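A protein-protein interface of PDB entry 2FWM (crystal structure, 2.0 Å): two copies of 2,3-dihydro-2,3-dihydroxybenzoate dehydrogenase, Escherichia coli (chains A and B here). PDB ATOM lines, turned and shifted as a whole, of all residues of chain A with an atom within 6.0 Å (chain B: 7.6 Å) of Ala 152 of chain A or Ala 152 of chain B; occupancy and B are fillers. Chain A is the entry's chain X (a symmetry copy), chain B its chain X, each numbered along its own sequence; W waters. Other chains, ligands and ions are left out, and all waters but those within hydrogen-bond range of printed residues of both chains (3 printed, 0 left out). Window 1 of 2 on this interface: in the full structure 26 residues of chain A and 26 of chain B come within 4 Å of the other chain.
The side-chain hydroxyl (OG) of Ser 155 of chain A lies close to the backbone carbonyl oxygen (O) of Gly 147 of chain B, 3.5 Å away.
The backbone NH of Ala 148 of chain B sits at hydrogen-bond distance from the side-chain hydroxyl of Ser 155 of chain A, 3.3 Å away.
The backbone carbonyl oxygen (O) of Gly 147 of chain A lies close to the side-chain hydroxyl (OG) of Ser 155 of chain B (3.5 Å).
OG of Ser 155 of chain B lies within hydrogen-bond range of N of Ala 148 of chain A (3.3 Å).
The backbone carbonyl oxygen of Phe 102 of chain B is in hydrogen-bond range of the backbone NH of Gly 107 of chain B (3.0 Å).
O of Ser 155 of chain B is in hydrogen-bond range of OG of Ser 159 of chain B (3.4 Å).
Among the printed residues, merely in contact across the chains: Ala 148 of chain A with Ala 152 of chain B (3.3 Å), Ala 152 of chain A with Ala 148 of chain B (3.3 Å), Val 106 of chain A with Trp 98 of chain B (3.6 Å), Ala 151 of chain A with Ser 155 of chain B (3.7 Å), Ser 155 of chain A with Ala 151 of chain B (3.7 Å), Val 106 of chain A with Phe 102 of chain B (3.8 Å), Phe 102 of chain A with Val 106 of chain B (3.8 Å), Ala 151 of chain A with Ala 151 of chain B (3.9 Å), Ala 152 of chain A with Ala 152 of chain B (3.9 Å), Ala 152 of chain A with Phe 102 of chain B (3.9 Å), Phe 102 of chain A with Ala 152 of chain B (3.9 Å) and Phe 102 of chain A with Phe 102 of chain B (3.9 Å).
Ala 152 of chain A touches three residues of chain B.
Ala 152 of chain B touches just these residues of chain A: Phe 102, Ala 148 and Ala 152.
Of the printed residues of chain B, Ala 151 of chain A touches Ala 151 (3.9 Å) and Ser 155 (3.7 Å).
Of the printed residues of chain B, Phe 102 of chain A touches Phe 102, Val 106 and Ala 152.
Printed residues of chain B within 4 Å of Val 106 of chain A: Trp 98 (3.6 Å) and Phe 102 (3.8 Å).
Of the printed residues of chain A, Ser 155 of chain B touches Gly 147 (3.5 Å), Ala 148 (3.3 Å) and Ala 151 (3.7 Å).
The nearest residue of chain B that does not touch Ala 152 of chain A is Ala 151 of chain B (4.5 Å).
The nearest residue of chain A that does not touch Ala 152 of chain B is Ala 151 of chain A (4.5 Å).
Of the 13 printed residues of chain A, 7 touch a printed residue of chain B.
Printed residues of chain A that touch a printed residue of chain B: Phe 102, Val 106, Gly 147, Ala 148, Ala 151, Ala 152 and Ser 155.
Hydrophobic or aromatic side chains of chain A that line the printed part of chain B: Phe 102, Val 106, Ala 148, Ala 151 and Ala 152.
Printed residues of chain B that touch a printed residue of chain A: Trp 98, Phe 102, Val 106, Gly 147, Ala 148, Ala 151, Ala 152 and Ser 155.
Among the printed residues, no Asp or Glu carboxylate lies within 4 Å of a Lys or Arg side-chain nitrogen of the other chain.
Phe 102 of chain A touches Ala 152 of chain B, and with the chains exchanged Ala 152 of chain A touches Phe 102 of chain B.
Ala 148 of chain A touches Ser 155 of chain B, and with the chains exchanged Ser 155 of chain A touches Ala 148 of chain B.
Ala 151 of chain B touches its own counterpart, Ala 151 of chain A.
Ala 151 of chain A touches Ser 155 of chain B, and with the chains exchanged Ser 155 of chain A touches Ala 151 of chain B.
Positions printed for both chains: 102, 106, 147, 148, 149, 150, 151, 152, 153, 154, 155, 156 and 157.
Water W3 bridges the side-chain hydroxyl of Ser 155 of chain A (2.5 Å) and the backbone carbonyl oxygen of Ala 136 of chain B (3.3 Å).
Water W2 lies within hydrogen-bond range of O of Ser 144 of chain B (2.7 Å), OG of Ser 155 of chain A (2.8 Å) and N of Ala 148 of chain B (3.2 Å).
Water W1 lies within hydrogen-bond range of the side-chain hydroxyl (OG) of Ser 159 of chain B, the side-chain hydroxyl (OG) of Ser 155 of chain B and the backbone NH (N) of Ala 148 of chain A.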
ATOM      1  N   PHE A 102      -1.003 -18.903 -30.894  1.00  0.00           N
ATOM      2  CA  PHE A 102      -0.614 -18.257 -29.645  1.00  0.00           C
ATOM      3  C   PHE A 102       0.894 -18.151 -29.476  1.00  0.00           C
ATOM      4  O   PHE A 102       1.389 -17.119 -29.006  1.00  0.00           O
ATOM      5  CB  PHE A 102      -1.287 -18.919 -28.441  1.00  0.00           C
ATOM      6  CG  PHE A 102      -2.706 -18.481 -28.253  1.00  0.00           C
ATOM      7  CD1 PHE A 102      -3.015 -17.414 -27.405  1.00  0.00           C
ATOM      8  CD2 PHE A 102      -3.734 -19.094 -28.960  1.00  0.00           C
ATOM      9  CE1 PHE A 102      -4.330 -16.988 -27.247  1.00  0.00           C
ATOM     10  CE2 PHE A 102      -5.049 -18.666 -28.813  1.00  0.00           C
ATOM     11  CZ  PHE A 102      -5.348 -17.607 -27.959  1.00  0.00           C
ATOM     12  N   VAL A 106       1.262 -14.157 -29.585  1.00  0.00           N
ATOM     13  CA  VAL A 106       1.403 -13.610 -28.230  1.00  0.00           C
ATOM     14  C   VAL A 106       2.796 -13.864 -27.664  1.00  0.00           C
ATOM     15  O   VAL A 106       3.442 -12.948 -27.150  1.00  0.00           O
ATOM     16  CB  VAL A 106       0.377 -14.191 -27.217  1.00  0.00           C
ATOM     17  CG1 VAL A 106       0.192 -13.213 -26.056  1.00  0.00           C
ATOM     18  CG2 VAL A 106      -0.957 -14.494 -27.883  1.00  0.00           C
ATOM     19  N   GLY A 147      -8.190 -13.903 -33.623  1.00  0.00           N
ATOM     20  CA  GLY A 147      -8.708 -12.735 -32.903  1.00  0.00           C
ATOM     21  C   GLY A 147      -8.385 -12.765 -31.423  1.00  0.00           C
ATOM     22  O   GLY A 147      -7.968 -11.747 -30.857  1.00  0.00           O
ATOM     23  N   ALA A 148      -8.572 -13.931 -30.800  1.00  0.00           N
ATOM     24  CA  ALA A 148      -8.220 -14.141 -29.383  1.00  0.00           C
ATOM     25  C   ALA A 148      -6.736 -13.902 -29.108  1.00  0.00           C
ATOM     26  O   ALA A 148      -6.388 -13.245 -28.119  1.00  0.00           O
ATOM     27  CB  ALA A 148      -8.624 -15.539 -28.920  1.00  0.00           C
ATOM     28  N   SER A 149      -5.871 -14.420 -29.981  1.00  0.00           N
ATOM     29  CA  SER A 149      -4.422 -14.244 -29.811  1.00  0.00           C
ATOM     30  C   SER A 149      -4.051 -12.773 -29.958  1.00  0.00           C
ATOM     31  O   SER A 149      -3.199 -12.262 -29.232  1.00  0.00           O
ATOM     32  CB  SER A 149      -3.615 -15.124 -30.780  1.00  0.00           C
ATOM     33  OG  SER A 149      -3.731 -14.692 -32.130  1.00  0.00           O
ATOM     34  N   LYS A 150      -4.731 -12.092 -30.873  1.00  0.00           N
ATOM     35  CA  LYS A 150      -4.469 -10.686 -31.141  1.00  0.00           C
ATOM     36  C   LYS A 150      -5.017  -9.780 -30.034  1.00  0.00           C
ATOM     37  O   LYS A 150      -4.453  -8.718 -29.768  1.00  0.00           O
ATOM     38  CB  LYS A 150      -5.005 -10.303 -32.530  1.00  0.00           C
ATOM     39  CG  LYS A 150      -4.236 -10.951 -33.708  1.00  0.00           C
ATOM     40  CD  LYS A 150      -2.772 -10.477 -33.761  1.00  0.00           C
ATOM     41  CE  LYS A 150      -2.192 -10.511 -35.185  1.00  0.00           C
ATOM     42  NZ  LYS A 150      -0.817  -9.912 -35.220  1.00  0.00           N
ATOM     43  N   ALA A 151      -6.106 -10.207 -29.383  1.00  0.00           N
ATOM     44  CA  ALA A 151      -6.595  -9.538 -28.162  1.00  0.00           C
ATOM     45  C   ALA A 151      -5.604  -9.670 -26.997  1.00  0.00           C
ATOM     46  O   ALA A 151      -5.342  -8.698 -26.293  1.00  0.00           O
ATOM     47  CB  ALA A 151      -7.993 -10.053 -27.765  1.00  0.00           C
ATOM     48  N   ALA A 152      -5.057 -10.869 -26.796  1.00  0.00           N
ATOM     49  CA  ALA A 152      -3.978 -11.078 -25.827  1.00  0.00           C
ATOM     50  C   ALA A 152      -2.764 -10.198 -26.123  1.00  0.00           C
ATOM     51  O   ALA A 152      -2.211  -9.576 -25.221  1.00  0.00           O
ATOM     52  CB  ALA A 152      -3.567 -12.541 -25.781  1.00  0.00           C
ATOM     53  N   LEU A 153      -2.362 -10.142 -27.386  1.00  0.00           N
ATOM     54  CA  LEU A 153      -1.238  -9.308 -27.804  1.00  0.00           C
ATOM     55  C   LEU A 153      -1.457  -7.826 -27.490  1.00  0.00           C
ATOM     56  O   LEU A 153      -0.560  -7.163 -26.951  1.00  0.00           O
ATOM     57  CB  LEU A 153      -0.957  -9.495 -29.295  1.00  0.00           C
ATOM     58  CG  LEU A 153       0.159  -8.632 -29.895  1.00  0.00           C
ATOM     59  CD1 LEU A 153       1.493  -8.935 -29.207  1.00  0.00           C
ATOM     60  CD2 LEU A 153       0.278  -8.859 -31.398  1.00  0.00           C
ATOM     61  N   LYS A 154      -2.638  -7.312 -27.823  1.00  0.00           N
ATOM     62  CA  LYS A 154      -2.970  -5.924 -27.519  1.00  0.00           C
ATOM     63  C   LYS A 154      -2.950  -5.662 -26.009  1.00  0.00           C
ATOM     64  O   LYS A 154      -2.381  -4.672 -25.553  1.00  0.00           O
ATOM     65  CB  LYS A 154      -4.333  -5.542 -28.087  1.00  0.00           C
ATOM     66  CG  LYS A 154      -4.748  -4.133 -27.668  1.00  0.00           C
ATOM     67  CD  LYS A 154      -6.198  -3.900 -27.834  1.00  0.00           C
ATOM     68  CE  LYS A 154      -6.567  -2.552 -27.272  1.00  0.00           C
ATOM     69  NZ  LYS A 154      -7.624  -2.019 -28.132  1.00  0.00           N
ATOM     70  N   SER A 155      -3.590  -6.549 -25.253  1.00  0.00           N
ATOM     71  CA  SER A 155      -3.609  -6.468 -23.791  1.00  0.00           C
ATOM     72  C   SER A 155      -2.183  -6.418 -23.235  1.00  0.00           C
ATOM     73  O   SER A 155      -1.865  -5.553 -22.426  1.00  0.00           O
ATOM     74  CB  SER A 155      -4.359  -7.671 -23.219  1.00  0.00           C
ATOM     75  OG  SER A 155      -4.377  -7.662 -21.799  1.00  0.00           O
ATOM     76  N   LEU A 156      -1.337  -7.352 -23.681  1.00  0.00           N
ATOM     77  CA  LEU A 156       0.060  -7.427 -23.236  1.00  0.00           C
ATOM     78  C   LEU A 156       0.824  -6.151 -23.572  1.00  0.00           C
ATOM     79  O   LEU A 156       1.592  -5.648 -22.748  1.00  0.00           O
ATOM     80  CB  LEU A 156       0.780  -8.625 -23.873  1.00  0.00           C
ATOM     81  CG  LEU A 156       2.271  -8.771 -23.519  1.00  0.00           C
ATOM     82  CD1 LEU A 156       2.432  -9.248 -22.064  1.00  0.00           C
ATOM     83  CD2 LEU A 156       2.935  -9.734 -24.478  1.00  0.00           C
ATOM     84  N   ALA A 157       0.622  -5.652 -24.789  1.00  0.00           N
ATOM     85  CA  ALA A 157       1.260  -4.418 -25.246  1.00  0.00           C
ATOM     86  C   ALA A 157       0.900  -3.207 -24.378  1.00  0.00           C
ATOM     87  O   ALA A 157       1.773  -2.404 -24.049  1.00  0.00           O
ATOM     88  CB  ALA A 157       0.934  -4.153 -26.721  1.00  0.00           C
ATOM     89  N   TRP B  98       4.101 -18.289 -17.738  1.00  0.00           N
ATOM     90  CA  TRP B  98       3.506 -17.782 -18.971  1.00  0.00           C
ATOM     91  C   TRP B  98       2.678 -18.868 -19.668  1.00  0.00           C
ATOM     92  O   TRP B  98       1.508 -18.652 -20.009  1.00  0.00           O
ATOM     93  CB  TRP B  98       4.596 -17.267 -19.915  1.00  0.00           C
ATOM     94  CG  TRP B  98       4.072 -16.899 -21.268  1.00  0.00           C
ATOM     95  CD1 TRP B  98       4.111 -17.663 -22.397  1.00  0.00           C
ATOM     96  CD2 TRP B  98       3.428 -15.673 -21.630  1.00  0.00           C
ATOM     97  NE1 TRP B  98       3.532 -16.985 -23.446  1.00  0.00           N
ATOM     98  CE2 TRP B  98       3.106 -15.760 -23.000  1.00  0.00           C
ATOM     99  CE3 TRP B  98       3.097 -14.502 -20.929  1.00  0.00           C
ATOM    100  CZ2 TRP B  98       2.465 -14.723 -23.684  1.00  0.00           C
ATOM    101  CZ3 TRP B  98       2.458 -13.475 -21.614  1.00  0.00           C
ATOM    102  CH2 TRP B  98       2.155 -13.593 -22.978  1.00  0.00           C
ATOM    103  N   PHE B 102      -1.681 -19.345 -20.064  1.00  0.00           N
ATOM    104  CA  PHE B 102      -2.420 -19.484 -21.314  1.00  0.00           C
ATOM    105  C   PHE B 102      -3.053 -20.857 -21.480  1.00  0.00           C
ATOM    106  O   PHE B 102      -4.193 -20.956 -21.952  1.00  0.00           O
ATOM    107  CB  PHE B 102      -1.560 -19.093 -22.517  1.00  0.00           C
ATOM    108  CG  PHE B 102      -1.466 -17.611 -22.710  1.00  0.00           C
ATOM    109  CD1 PHE B 102      -2.353 -16.948 -23.562  1.00  0.00           C
ATOM    110  CD2 PHE B 102      -0.530 -16.866 -22.003  1.00  0.00           C
ATOM    111  CE1 PHE B 102      -2.285 -15.567 -23.724  1.00  0.00           C
ATOM    112  CE2 PHE B 102      -0.464 -15.485 -22.154  1.00  0.00           C
ATOM    113  CZ  PHE B 102      -1.346 -14.832 -23.013  1.00  0.00           C
ATOM    114  N   ASN B 105      -6.046 -20.640 -18.844  1.00  0.00           N
ATOM    115  CA  ASN B 105      -6.992 -19.520 -18.963  1.00  0.00           C
ATOM    116  C   ASN B 105      -7.627 -19.367 -20.342  1.00  0.00           C
ATOM    117  O   ASN B 105      -8.755 -18.877 -20.452  1.00  0.00           O
ATOM    118  CB  ASN B 105      -6.371 -18.192 -18.505  1.00  0.00           C
ATOM    119  CG  ASN B 105      -6.054 -18.178 -17.020  1.00  0.00           C
ATOM    120  OD1 ASN B 105      -6.414 -19.103 -16.288  1.00  0.00           O
ATOM    121  ND2 ASN B 105      -5.365 -17.134 -16.569  1.00  0.00           N
ATOM    122  N   VAL B 106      -6.919 -19.786 -21.382  1.00  0.00           N
ATOM    123  CA  VAL B 106      -7.477 -19.728 -22.739  1.00  0.00           C
ATOM    124  C   VAL B 106      -7.732 -21.123 -23.301  1.00  0.00           C
ATOM    125  O   VAL B 106      -8.816 -21.404 -23.817  1.00  0.00           O
ATOM    126  CB  VAL B 106      -6.568 -18.978 -23.753  1.00  0.00           C
ATOM    127  CG1 VAL B 106      -7.414 -18.462 -24.917  1.00  0.00           C
ATOM    128  CG2 VAL B 106      -5.813 -17.835 -23.088  1.00  0.00           C
ATOM    129  N   GLY B 107      -6.717 -21.984 -23.228  1.00  0.00           N
ATOM    130  CA  GLY B 107      -6.812 -23.312 -23.813  1.00  0.00           C
ATOM    131  C   GLY B 107      -7.937 -24.121 -23.203  1.00  0.00           C
ATOM    132  O   GLY B 107      -8.559 -24.944 -23.878  1.00  0.00           O
ATOM    133  N   ALA B 132     -13.951 -14.142 -17.009  1.00  0.00           N
ATOM    134  CA  ALA B 132     -12.690 -13.528 -17.398  1.00  0.00           C
ATOM    135  C   ALA B 132     -12.099 -12.801 -16.182  1.00  0.00           C
ATOM    136  O   ALA B 132     -11.889 -13.417 -15.141  1.00  0.00           O
ATOM    137  CB  ALA B 132     -12.897 -12.587 -18.585  1.00  0.00           C
ATOM    138  N   ALA B 136      -8.548  -7.979 -17.899  1.00  0.00           N
ATOM    139  CA  ALA B 136      -8.704  -8.013 -19.349  1.00  0.00           C
ATOM    140  C   ALA B 136      -9.172  -6.660 -19.910  1.00  0.00           C
ATOM    141  O   ALA B 136      -9.162  -6.453 -21.122  1.00  0.00           O
ATOM    142  CB  ALA B 136      -9.691  -9.122 -19.746  1.00  0.00           C
ATOM    143  N   SER B 144       0.313  -8.608 -16.229  1.00  0.00           N
ATOM    144  CA  SER B 144       0.402  -8.531 -17.697  1.00  0.00           C
ATOM    145  C   SER B 144      -0.009  -9.827 -18.405  1.00  0.00           C
ATOM    146  O   SER B 144      -0.839  -9.785 -19.311  1.00  0.00           O
ATOM    147  CB  SER B 144       1.787  -8.072 -18.162  1.00  0.00           C
ATOM    148  OG  SER B 144       2.767  -9.058 -17.912  1.00  0.00           O
ATOM    149  N   ALA B 145       0.549 -10.968 -17.993  1.00  0.00           N
ATOM    150  CA  ALA B 145       0.217 -12.256 -18.627  1.00  0.00           C
ATOM    151  C   ALA B 145      -1.203 -12.717 -18.307  1.00  0.00           C
ATOM    152  O   ALA B 145      -1.925 -13.177 -19.193  1.00  0.00           O
ATOM    153  CB  ALA B 145       1.223 -13.343 -18.243  1.00  0.00           C
ATOM    154  N   TYR B 146      -1.581 -12.597 -17.037  1.00  0.00           N
ATOM    155  CA  TYR B 146      -2.919 -12.947 -16.574  1.00  0.00           C
ATOM    156  C   TYR B 146      -3.980 -12.161 -17.338  1.00  0.00           C
ATOM    157  O   TYR B 146      -4.918 -12.748 -17.898  1.00  0.00           O
ATOM    158  CB  TYR B 146      -3.044 -12.691 -15.071  1.00  0.00           C
ATOM    159  CG  TYR B 146      -4.413 -12.992 -14.499  1.00  0.00           C
ATOM    160  CD1 TYR B 146      -4.849 -14.311 -14.330  1.00  0.00           C
ATOM    161  CD2 TYR B 146      -5.269 -11.964 -14.111  1.00  0.00           C
ATOM    162  CE1 TYR B 146      -6.096 -14.590 -13.802  1.00  0.00           C
ATOM    163  CE2 TYR B 146      -6.526 -12.236 -13.586  1.00  0.00           C
ATOM    164  CZ  TYR B 146      -6.927 -13.548 -13.429  1.00  0.00           C
ATOM    165  OH  TYR B 146      -8.161 -13.821 -12.899  1.00  0.00           O
ATOM    166  N   GLY B 147      -3.816 -10.844 -17.367  1.00  0.00           N
ATOM    167  CA  GLY B 147      -4.722  -9.948 -18.092  1.00  0.00           C
ATOM    168  C   GLY B 147      -4.806 -10.266 -19.571  1.00  0.00           C
ATOM    169  O   GLY B 147      -5.905 -10.296 -20.140  1.00  0.00           O
ATOM    170  N   ALA B 148      -3.648 -10.506 -20.190  1.00  0.00           N
ATOM    171  CA  ALA B 148      -3.573 -10.914 -21.606  1.00  0.00           C
ATOM    172  C   ALA B 148      -4.322 -12.218 -21.878  1.00  0.00           C
ATOM    173  O   ALA B 148      -5.058 -12.314 -22.869  1.00  0.00           O
ATOM    174  CB  ALA B 148      -2.122 -11.033 -22.066  1.00  0.00           C
ATOM    175  N   SER B 149      -4.146 -13.207 -21.002  1.00  0.00           N
ATOM    176  CA  SER B 149      -4.823 -14.500 -21.169  1.00  0.00           C
ATOM    177  C   SER B 149      -6.331 -14.326 -21.026  1.00  0.00           C
ATOM    178  O   SER B 149      -7.109 -14.944 -21.752  1.00  0.00           O
ATOM    179  CB  SER B 149      -4.289 -15.564 -20.195  1.00  0.00           C
ATOM    180  OG  SER B 149      -4.654 -15.298 -18.848  1.00  0.00           O
ATOM    181  N   LYS B 150      -6.729 -13.445 -20.115  1.00  0.00           N
ATOM    182  CA  LYS B 150      -8.137 -13.192 -19.851  1.00  0.00           C
ATOM    183  C   LYS B 150      -8.788 -12.362 -20.963  1.00  0.00           C
ATOM    184  O   LYS B 150      -9.980 -12.514 -21.230  1.00  0.00           O
ATOM    185  CB  LYS B 150      -8.309 -12.550 -18.464  1.00  0.00           C
ATOM    186  CG  LYS B 150      -7.978 -13.495 -17.282  1.00  0.00           C
ATOM    187  CD  LYS B 150      -8.940 -14.696 -17.228  1.00  0.00           C
ATOM    188  CE  LYS B 150      -9.117 -15.245 -15.802  1.00  0.00           C
ATOM    189  NZ  LYS B 150     -10.164 -16.319 -15.767  1.00  0.00           N
ATOM    190  N   ALA B 151      -8.001 -11.497 -21.615  1.00  0.00           N
ATOM    191  CA  ALA B 151      -8.451 -10.807 -22.838  1.00  0.00           C
ATOM    192  C   ALA B 151      -8.676 -11.784 -24.001  1.00  0.00           C
ATOM    193  O   ALA B 151      -9.676 -11.686 -24.707  1.00  0.00           O
ATOM    194  CB  ALA B 151      -7.473  -9.683 -23.237  1.00  0.00           C
ATOM    195  N   ALA B 152      -7.748 -12.721 -24.196  1.00  0.00           N
ATOM    196  CA  ALA B 152      -7.932 -13.807 -25.163  1.00  0.00           C
ATOM    197  C   ALA B 152      -9.187 -14.630 -24.866  1.00  0.00           C
ATOM    198  O   ALA B 152      -9.962 -14.929 -25.769  1.00  0.00           O
ATOM    199  CB  ALA B 152      -6.710 -14.709 -25.203  1.00  0.00           C
ATOM    200  N   LEU B 153      -9.384 -14.982 -23.603  1.00  0.00           N
ATOM    201  CA  LEU B 153     -10.563 -15.736 -23.185  1.00  0.00           C
ATOM    202  C   LEU B 153     -11.871 -15.007 -23.504  1.00  0.00           C
ATOM    203  O   LEU B 153     -12.807 -15.612 -24.044  1.00  0.00           O
ATOM    204  CB  LEU B 153     -10.491 -16.060 -21.693  1.00  0.00           C
ATOM    205  CG  LEU B 153     -11.695 -16.796 -21.094  1.00  0.00           C
ATOM    206  CD1 LEU B 153     -11.883 -18.153 -21.777  1.00  0.00           C
ATOM    207  CD2 LEU B 153     -11.528 -16.983 -19.589  1.00  0.00           C
ATOM    208  N   LYS B 154     -11.934 -13.719 -23.176  1.00  0.00           N
ATOM    209  CA  LYS B 154     -13.113 -12.918 -23.485  1.00  0.00           C
ATOM    210  C   LYS B 154     -13.362 -12.849 -24.995  1.00  0.00           C
ATOM    211  O   LYS B 154     -14.489 -13.031 -25.454  1.00  0.00           O
ATOM    212  CB  LYS B 154     -12.989 -11.506 -22.921  1.00  0.00           C
ATOM    213  CG  LYS B 154     -14.158 -10.620 -23.345  1.00  0.00           C
ATOM    214  CD  LYS B 154     -13.862  -9.181 -23.184  1.00  0.00           C
ATOM    215  CE  LYS B 154     -14.992  -8.361 -23.751  1.00  0.00           C
ATOM    216  NZ  LYS B 154     -15.117  -7.180 -22.896  1.00  0.00           N
ATOM    217  N   SER B 155     -12.304 -12.567 -25.750  1.00  0.00           N
ATOM    218  CA  SER B 155     -12.370 -12.526 -27.213  1.00  0.00           C
ATOM    219  C   SER B 155     -12.920 -13.843 -27.765  1.00  0.00           C
ATOM    220  O   SER B 155     -13.840 -13.837 -28.576  1.00  0.00           O
ATOM    221  CB  SER B 155     -10.977 -12.252 -27.783  1.00  0.00           C
ATOM    222  OG  SER B 155     -10.977 -12.237 -29.202  1.00  0.00           O
ATOM    223  N   LEU B 156     -12.348 -14.963 -27.315  1.00  0.00           N
ATOM    224  CA  LEU B 156     -12.772 -16.298 -27.756  1.00  0.00           C
ATOM    225  C   LEU B 156     -14.237 -16.559 -27.422  1.00  0.00           C
ATOM    226  O   LEU B 156     -14.977 -17.101 -28.247  1.00  0.00           O
ATOM    227  CB  LEU B 156     -11.909 -17.393 -27.113  1.00  0.00           C
ATOM    228  CG  LEU B 156     -12.299 -18.841 -27.464  1.00  0.00           C
ATOM    229  CD1 LEU B 156     -11.907 -19.165 -28.917  1.00  0.00           C
ATOM    230  CD2 LEU B 156     -11.636 -19.799 -26.501  1.00  0.00           C
ATOM    231  N   ALA B 157     -14.634 -16.189 -26.208  1.00  0.00           N
ATOM    232  CA  ALA B 157     -16.016 -16.347 -25.754  1.00  0.00           C
ATOM    233  C   ALA B 157     -17.018 -15.584 -26.626  1.00  0.00           C
ATOM    234  O   ALA B 157     -18.078 -16.117 -26.955  1.00  0.00           O
ATOM    235  CB  ALA B 157     -16.151 -15.943 -24.280  1.00  0.00           C
ATOM    236  N   LEU B 158     -16.698 -14.348 -27.004  1.00  0.00           N
ATOM    237  CA  LEU B 158     -17.605 -13.581 -27.870  1.00  0.00           C
ATOM    238  C   LEU B 158     -17.639 -14.128 -29.298  1.00  0.00           C
ATOM    239  O   LEU B 158     -18.683 -14.101 -29.953  1.00  0.00           O
ATOM    240  CB  LEU B 158     -17.273 -12.075 -27.875  1.00  0.00           C
ATOM    241  CG  LEU B 158     -17.254 -11.258 -26.571  1.00  0.00           C
ATOM    242  CD1 LEU B 158     -17.553  -9.767 -26.870  1.00  0.00           C
ATOM    243  CD2 LEU B 158     -18.190 -11.786 -25.503  1.00  0.00           C
ATOM    244  N   SER B 159     -16.497 -14.623 -29.771  1.00  0.00           N
ATOM    245  CA  SER B 159     -16.417 -15.266 -31.078  1.00  0.00           C
ATOM    246  C   SER B 159     -17.266 -16.536 -31.157  1.00  0.00           C
ATOM    247  O   SER B 159     -17.989 -16.743 -32.134  1.00  0.00           O
ATOM    248  CB  SER B 159     -14.959 -15.541 -31.464  1.00  0.00           C
ATOM    249  OG  SER B 159     -14.328 -14.333 -31.879  1.00  0.00           O
HETATM  250  O   HOH W   1     -11.723 -14.197 -31.053  1.00  0.00           O
HETATM  251  O   HOH W   2      -2.284  -7.652 -19.943  1.00  0.00           O
HETATM  252  O   HOH W   3      -5.902  -6.054 -20.560  1.00  0.00           O
